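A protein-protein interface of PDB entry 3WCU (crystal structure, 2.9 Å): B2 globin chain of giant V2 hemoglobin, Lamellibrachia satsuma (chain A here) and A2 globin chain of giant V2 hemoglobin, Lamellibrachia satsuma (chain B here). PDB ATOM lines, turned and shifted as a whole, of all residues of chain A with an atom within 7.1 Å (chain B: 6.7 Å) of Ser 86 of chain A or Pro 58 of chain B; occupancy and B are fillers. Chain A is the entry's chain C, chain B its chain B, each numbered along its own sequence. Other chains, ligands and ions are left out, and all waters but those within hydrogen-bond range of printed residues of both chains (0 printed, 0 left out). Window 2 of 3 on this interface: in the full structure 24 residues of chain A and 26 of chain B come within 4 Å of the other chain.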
ATOM      1  N   LEU A  81      10.724   4.470   4.756  1.00  0.00           N
ATOM      2  CA  LEU A  81      11.444   4.318   3.499  1.00  0.00           C
ATOM      3  C   LEU A  81      11.238   5.509   2.551  1.00  0.00           C
ATOM      4  O   LEU A  81      11.878   5.593   1.500  1.00  0.00           O
ATOM      5  CB  LEU A  81      11.040   2.999   2.820  1.00  0.00           C
ATOM      6  CG  LEU A  81      11.853   1.763   3.215  1.00  0.00           C
ATOM      7  CD1 LEU A  81      13.164   1.811   2.488  1.00  0.00           C
ATOM      8  CD2 LEU A  81      12.063   1.704   4.733  1.00  0.00           C
ATOM      9  N   SER A  83      12.317   8.060   3.021  1.00  0.00           N
ATOM     10  CA  SER A  83      13.625   8.691   3.121  1.00  0.00           C
ATOM     11  C   SER A  83      14.625   8.115   2.128  1.00  0.00           C
ATOM     12  O   SER A  83      15.648   8.737   1.859  1.00  0.00           O
ATOM     13  CB  SER A  83      14.182   8.549   4.541  1.00  0.00           C
ATOM     14  OG  SER A  83      13.625   9.520   5.412  1.00  0.00           O
ATOM     15  N   ASP A  84      14.344   6.926   1.600  1.00  0.00           N
ATOM     16  CA  ASP A  84      15.220   6.284   0.616  1.00  0.00           C
ATOM     17  C   ASP A  84      14.363   5.654  -0.469  1.00  0.00           C
ATOM     18  O   ASP A  84      14.270   4.436  -0.556  1.00  0.00           O
ATOM     19  CB  ASP A  84      16.078   5.220   1.289  1.00  0.00           C
ATOM     20  CG  ASP A  84      16.955   5.795   2.385  1.00  0.00           C
ATOM     21  OD1 ASP A  84      17.960   6.474   2.074  1.00  0.00           O
ATOM     22  OD2 ASP A  84      16.632   5.579   3.570  1.00  0.00           O
ATOM     23  N   PRO A  85      13.727   6.482  -1.315  1.00  0.00           N
ATOM     24  CA  PRO A  85      12.866   6.003  -2.396  1.00  0.00           C
ATOM     25  C   PRO A  85      13.358   4.827  -3.256  1.00  0.00           C
ATOM     26  O   PRO A  85      12.567   3.938  -3.568  1.00  0.00           O
ATOM     27  CB  PRO A  85      12.559   7.280  -3.204  1.00  0.00           C
ATOM     28  CG  PRO A  85      13.578   8.285  -2.740  1.00  0.00           C
ATOM     29  CD  PRO A  85      13.759   7.953  -1.295  1.00  0.00           C
ATOM     30  N   SER A  86      14.630   4.796  -3.653  1.00  0.00           N
ATOM     31  CA  SER A  86      15.101   3.657  -4.451  1.00  0.00           C
ATOM     32  C   SER A  86      14.684   2.379  -3.741  1.00  0.00           C
ATOM     33  O   SER A  86      14.073   1.506  -4.342  1.00  0.00           O
ATOM     34  CB  SER A  86      16.620   3.669  -4.613  1.00  0.00           C
ATOM     35  OG  SER A  86      17.023   4.617  -5.583  1.00  0.00           O
ATOM     36  N   THR A  87      14.995   2.291  -2.453  1.00  0.00           N
ATOM     37  CA  THR A  87      14.635   1.119  -1.663  1.00  0.00           C
ATOM     38  C   THR A  87      13.131   0.972  -1.502  1.00  0.00           C
ATOM     39  O   THR A  87      12.603  -0.116  -1.625  1.00  0.00           O
ATOM     40  CB  THR A  87      15.236   1.165  -0.260  1.00  0.00           C
ATOM     41  OG1 THR A  87      16.662   1.300  -0.344  1.00  0.00           O
ATOM     42  CG2 THR A  87      14.904  -0.094   0.480  1.00  0.00           C
ATOM     43  N   LEU A  88      12.436   2.064  -1.218  1.00  0.00           N
ATOM     44  CA  LEU A  88      10.990   1.997  -1.037  1.00  0.00           C
ATOM     45  C   LEU A  88      10.270   1.415  -2.259  1.00  0.00           C
ATOM     46  O   LEU A  88       9.208   0.803  -2.127  1.00  0.00           O
ATOM     47  CB  LEU A  88      10.428   3.386  -0.722  1.00  0.00           C
ATOM     48  CG  LEU A  88       8.902   3.469  -0.792  1.00  0.00           C
ATOM     49  CD1 LEU A  88       8.345   2.737   0.407  1.00  0.00           C
ATOM     50  CD2 LEU A  88       8.417   4.903  -0.822  1.00  0.00           C
ATOM     51  N   ASN A  89      10.831   1.607  -3.450  1.00  0.00           N
ATOM     52  CA  ASN A  89      10.188   1.070  -4.640  1.00  0.00           C
ATOM     53  C   ASN A  89      10.325  -0.444  -4.644  1.00  0.00           C
ATOM     54  O   ASN A  89       9.341  -1.152  -4.828  1.00  0.00           O
ATOM     55  CB  ASN A  89      10.794   1.660  -5.914  1.00  0.00           C
ATOM     56  CG  ASN A  89      10.448   3.126  -6.098  1.00  0.00           C
ATOM     57  OD1 ASN A  89       9.329   3.551  -5.827  1.00  0.00           O
ATOM     58  ND2 ASN A  89      11.409   3.906  -6.577  1.00  0.00           N
ATOM     59  N   GLU A  90      11.542  -0.937  -4.427  1.00  0.00           N
ATOM     60  CA  GLU A  90      11.791  -2.375  -4.386  1.00  0.00           C
ATOM     61  C   GLU A  90      10.916  -2.995  -3.321  1.00  0.00           C
ATOM     62  O   GLU A  90      10.464  -4.129  -3.457  1.00  0.00           O
ATOM     63  CB  GLU A  90      13.252  -2.673  -4.046  1.00  0.00           C
ATOM     64  CG  GLU A  90      14.212  -2.443  -5.191  1.00  0.00           C
ATOM     65  CD  GLU A  90      13.914  -3.347  -6.362  1.00  0.00           C
ATOM     66  OE1 GLU A  90      14.023  -4.576  -6.193  1.00  0.00           O
ATOM     67  OE2 GLU A  90      13.564  -2.832  -7.445  1.00  0.00           O
ATOM     68  N   GLN A  91      10.679  -2.242  -2.257  1.00  0.00           N
ATOM     69  CA  GLN A  91       9.876  -2.726  -1.150  1.00  0.00           C
ATOM     70  C   GLN A  91       8.381  -2.591  -1.381  1.00  0.00           C
ATOM     71  O   GLN A  91       7.596  -3.370  -0.841  1.00  0.00           O
ATOM     72  CB  GLN A  91      10.267  -1.994   0.128  1.00  0.00           C
ATOM     73  CG  GLN A  91       9.389  -2.316   1.320  1.00  0.00           C
ATOM     74  CD  GLN A  91       9.308  -3.799   1.600  1.00  0.00           C
ATOM     75  OE1 GLN A  91      10.255  -4.545   1.328  1.00  0.00           O
ATOM     76  NE2 GLN A  91       8.181  -4.238   2.166  1.00  0.00           N
ATOM     77  N   ARG A 139       0.910   7.833  -2.214  1.00  0.00           N
ATOM     78  CA  ARG A 139       2.174   7.555  -2.880  1.00  0.00           C
ATOM     79  C   ARG A 139       2.591   6.119  -2.578  1.00  0.00           C
ATOM     80  O   ARG A 139       3.141   5.430  -3.431  1.00  0.00           O
ATOM     81  CB  ARG A 139       3.239   8.531  -2.376  1.00  0.00           C
ATOM     82  CG  ARG A 139       4.659   8.089  -2.597  1.00  0.00           C
ATOM     83  CD  ARG A 139       4.904   7.832  -4.046  1.00  0.00           C
ATOM     84  NE  ARG A 139       6.263   7.359  -4.275  1.00  0.00           N
ATOM     85  CZ  ARG A 139       6.781   6.269  -3.722  1.00  0.00           C
ATOM     86  NH1 ARG A 139       6.050   5.529  -2.896  1.00  0.00           N
ATOM     87  NH2 ARG A 139       8.028   5.916  -4.010  1.00  0.00           N
ATOM     88  N   ASN B  54      25.418  -8.205  -2.878  1.00  0.00           N
ATOM     89  CA  ASN B  54      25.724  -6.778  -2.698  1.00  0.00           C
ATOM     90  C   ASN B  54      24.652  -6.144  -1.807  1.00  0.00           C
ATOM     91  O   ASN B  54      23.566  -5.790  -2.278  1.00  0.00           O
ATOM     92  CB  ASN B  54      25.760  -6.097  -4.081  1.00  0.00           C
ATOM     93  CG  ASN B  54      25.825  -4.599  -3.993  1.00  0.00           C
ATOM     94  OD1 ASN B  54      24.894  -3.963  -3.514  1.00  0.00           O
ATOM     95  ND2 ASN B  54      26.928  -4.022  -4.454  1.00  0.00           N
ATOM     96  N   ILE B  55      24.963  -6.031  -0.517  1.00  0.00           N
ATOM     97  CA  ILE B  55      24.045  -5.467   0.471  1.00  0.00           C
ATOM     98  C   ILE B  55      23.874  -3.955   0.336  1.00  0.00           C
ATOM     99  O   ILE B  55      23.365  -3.299   1.244  1.00  0.00           O
ATOM    100  CB  ILE B  55      24.514  -5.781   1.922  1.00  0.00           C
ATOM    101  CG1 ILE B  55      25.975  -5.361   2.115  1.00  0.00           C
ATOM    102  CG2 ILE B  55      24.372  -7.256   2.211  1.00  0.00           C
ATOM    103  CD1 ILE B  55      26.563  -5.758   3.464  1.00  0.00           C
ATOM    104  N   TYR B  56      24.298  -3.410  -0.802  1.00  0.00           N
ATOM    105  CA  TYR B  56      24.208  -1.979  -1.080  1.00  0.00           C
ATOM    106  C   TYR B  56      23.039  -1.634  -2.002  1.00  0.00           C
ATOM    107  O   TYR B  56      22.567  -0.499  -2.015  1.00  0.00           O
ATOM    108  CB  TYR B  56      25.505  -1.496  -1.727  1.00  0.00           C
ATOM    109  CG  TYR B  56      26.703  -1.501  -0.805  1.00  0.00           C
ATOM    110  CD1 TYR B  56      26.875  -0.513   0.159  1.00  0.00           C
ATOM    111  CD2 TYR B  56      27.667  -2.497  -0.888  1.00  0.00           C
ATOM    112  CE1 TYR B  56      27.985  -0.517   1.019  1.00  0.00           C
ATOM    113  CE2 TYR B  56      28.779  -2.509  -0.027  1.00  0.00           C
ATOM    114  CZ  TYR B  56      28.931  -1.516   0.920  1.00  0.00           C
ATOM    115  OH  TYR B  56      30.025  -1.531   1.758  1.00  0.00           O
ATOM    116  N   THR B  57      22.586  -2.623  -2.769  1.00  0.00           N
ATOM    117  CA  THR B  57      21.484  -2.466  -3.729  1.00  0.00           C
ATOM    118  C   THR B  57      20.127  -2.226  -3.063  1.00  0.00           C
ATOM    119  O   THR B  57      19.921  -2.578  -1.901  1.00  0.00           O
ATOM    120  CB  THR B  57      21.349  -3.734  -4.628  1.00  0.00           C
ATOM    121  OG1 THR B  57      20.946  -4.853  -3.827  1.00  0.00           O
ATOM    122  CG2 THR B  57      22.672  -4.071  -5.285  1.00  0.00           C
ATOM    123  N   PRO B  58      19.186  -1.607  -3.790  1.00  0.00           N
ATOM    124  CA  PRO B  58      17.870  -1.363  -3.196  1.00  0.00           C
ATOM    125  C   PRO B  58      17.215  -2.688  -2.812  1.00  0.00           C
ATOM    126  O   PRO B  58      16.865  -2.911  -1.650  1.00  0.00           O
ATOM    127  CB  PRO B  58      17.113  -0.645  -4.314  1.00  0.00           C
ATOM    128  CG  PRO B  58      18.189   0.148  -4.971  1.00  0.00           C
ATOM    129  CD  PRO B  58      19.336  -0.856  -5.049  1.00  0.00           C
ATOM    130  N   ALA B  59      17.069  -3.563  -3.804  1.00  0.00           N
ATOM    131  CA  ALA B  59      16.454  -4.869  -3.614  1.00  0.00           C
ATOM    132  C   ALA B  59      16.797  -5.505  -2.272  1.00  0.00           C
ATOM    133  O   ALA B  59      15.919  -6.028  -1.577  1.00  0.00           O
ATOM    134  CB  ALA B  59      16.870  -5.778  -4.723  1.00  0.00           C
ATOM    135  N   PHE B  60      18.072  -5.463  -1.904  1.00  0.00           N
ATOM    136  CA  PHE B  60      18.479  -6.049  -0.640  1.00  0.00           C
ATOM    137  C   PHE B  60      18.129  -5.212   0.582  1.00  0.00           C
ATOM    138  O   PHE B  60      17.716  -5.747   1.613  1.00  0.00           O
ATOM    139  CB  PHE B  60      19.976  -6.316  -0.607  1.00  0.00           C
ATOM    140  CG  PHE B  60      20.428  -6.901   0.687  1.00  0.00           C
ATOM    141  CD1 PHE B  60      20.044  -8.185   1.049  1.00  0.00           C
ATOM    142  CD2 PHE B  60      21.159  -6.148   1.582  1.00  0.00           C
ATOM    143  CE1 PHE B  60      20.386  -8.706   2.294  1.00  0.00           C
ATOM    144  CE2 PHE B  60      21.503  -6.655   2.826  1.00  0.00           C
ATOM    145  CZ  PHE B  60      21.119  -7.934   3.188  1.00  0.00           C
ATOM    146  N   ARG B  61      18.332  -3.900   0.481  1.00  0.00           N
ATOM    147  CA  ARG B  61      18.032  -3.008   1.591  1.00  0.00           C
ATOM    148  C   ARG B  61      16.559  -3.173   1.885  1.00  0.00           C
ATOM    149  O   ARG B  61      16.136  -3.133   3.043  1.00  0.00           O
ATOM    150  CB  ARG B  61      18.363  -1.561   1.226  1.00  0.00           C
ATOM    151  CG  ARG B  61      19.852  -1.279   1.113  1.00  0.00           C
ATOM    152  CD  ARG B  61      20.068   0.128   0.615  1.00  0.00           C
ATOM    153  NE  ARG B  61      21.475   0.472   0.384  1.00  0.00           N
ATOM    154  CZ  ARG B  61      22.372   0.723   1.340  1.00  0.00           C
ATOM    155  NH1 ARG B  61      23.623   1.034   1.012  1.00  0.00           N
ATOM    156  NH2 ARG B  61      22.025   0.666   2.621  1.00  0.00           N
ATOM    157  N   ALA B  62      15.781  -3.386   0.828  1.00  0.00           N
ATOM    158  CA  ALA B  62      14.350  -3.594   0.986  1.00  0.00           C
ATOM    159  C   ALA B  62      14.157  -4.879   1.795  1.00  0.00           C
ATOM    160  O   ALA B  62      13.249  -4.964   2.631  1.00  0.00           O
ATOM    161  CB  ALA B  62      13.674  -3.712  -0.374  1.00  0.00           C
ATOM    162  N   HIS B  63      15.019  -5.869   1.549  1.00  0.00           N
ATOM    163  CA  HIS B  63      14.947  -7.134   2.280  1.00  0.00           C
ATOM    164  C   HIS B  63      15.212  -6.893   3.761  1.00  0.00           C
ATOM    165  O   HIS B  63      14.373  -7.225   4.617  1.00  0.00           O
ATOM    166  CB  HIS B  63      15.975  -8.147   1.747  1.00  0.00           C
ATOM    167  CG  HIS B  63      16.191  -9.319   2.656  1.00  0.00           C
ATOM    168  ND1 HIS B  63      15.193 -10.224   2.952  1.00  0.00           N
ATOM    169  CD2 HIS B  63      17.258  -9.673   3.412  1.00  0.00           C
ATOM    170  CE1 HIS B  63      15.636 -11.079   3.858  1.00  0.00           C
ATOM    171  NE2 HIS B  63      16.885 -10.766   4.156  1.00  0.00           N
ATOM    172  N   ALA B  64      16.386  -6.327   4.054  1.00  0.00           N
ATOM    173  CA  ALA B  64      16.782  -6.022   5.432  1.00  0.00           C
ATOM    174  C   ALA B  64      15.698  -5.186   6.107  1.00  0.00           C
ATOM    175  O   ALA B  64      15.453  -5.329   7.306  1.00  0.00           O
ATOM    176  CB  ALA B  64      18.123  -5.277   5.463  1.00  0.00           C
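The backbone carbonyl oxygen (O) of Tyr 56 of chain B lies within hydrogen-bond range of the guanidinium group (NE) of Arg 61 of chain B, at 2.8 Å.
CB of Pro 58 of chain B touches O of Ser 86 of chain A, at 3.7 Å. Thr 87 of chain A touches Arg 61 of chain B (OG1 to CB, 3.7 Å). Thr 87 of chain A touches Ala 62 of chain B (CG2 to N, 3.4 Å). CG of Glu 90 of chain A touches CB of Pro 58 of chain B, at 3.5 Å. Ala 59 of chain B touches Glu 90 of chain A (N to CG, 3.4 Å). CB of Glu 90 of chain A touches CB of Ala 62 of chain B, 3.8 Å away.
OE1 of Gln 91 of chain A lies close to O of Ala 62 of chain B (3.3 Å).
Hydrophobic or aromatic side chains of chain B that line the printed part of chain A: Pro 58, Ala 59 and Ala 62. Among the printed residues, 7 pairs touch across the chains. Among the printed residues, no Asp or Glu carboxylate lies within 4 Å of a Lys or Arg side-chain nitrogen of the other chain.
Of chain B, only Pro 58 (3.7 Å) comes within 4 Å of Ser 86 of chain A. Leu 88 of chain A touches none of the printed residues of chain B. Of the printed residues of chain B, Glu 90 of chain A touches Pro 58 (3.5 Å), Ala 59 (3.4 Å) and Ala 62 (3.8 Å). Of chain A, only Ser 86 (3.7 Å) and Glu 90 (3.5 Å) come within 4 Å of Pro 58 of chain B. Printed residues of chain A within 4 Å of Ala 59 of chain B: Glu 90 (3.4 Å). Of the printed residues of chain A, Arg 61 of chain B touches Thr 87 (3.7 Å). Printed residues of chain A within 4 Å of Ala 62 of chain B: Thr 87 (3.4 Å), Glu 90 (3.8 Å) and Gln 91 (3.3 Å). The nearest residue of chain B that does not touch Ser 86 of chain A is Ala 59 of chain B (5.9 Å). The nearest residue of chain A that does not touch Pro 58 of chain B is Thr 87 of chain A (4.03 Å). The nearest printed residue of chain A that does not touch Ala 62 of chain B is Leu 81 of chain A (5.7 Å).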
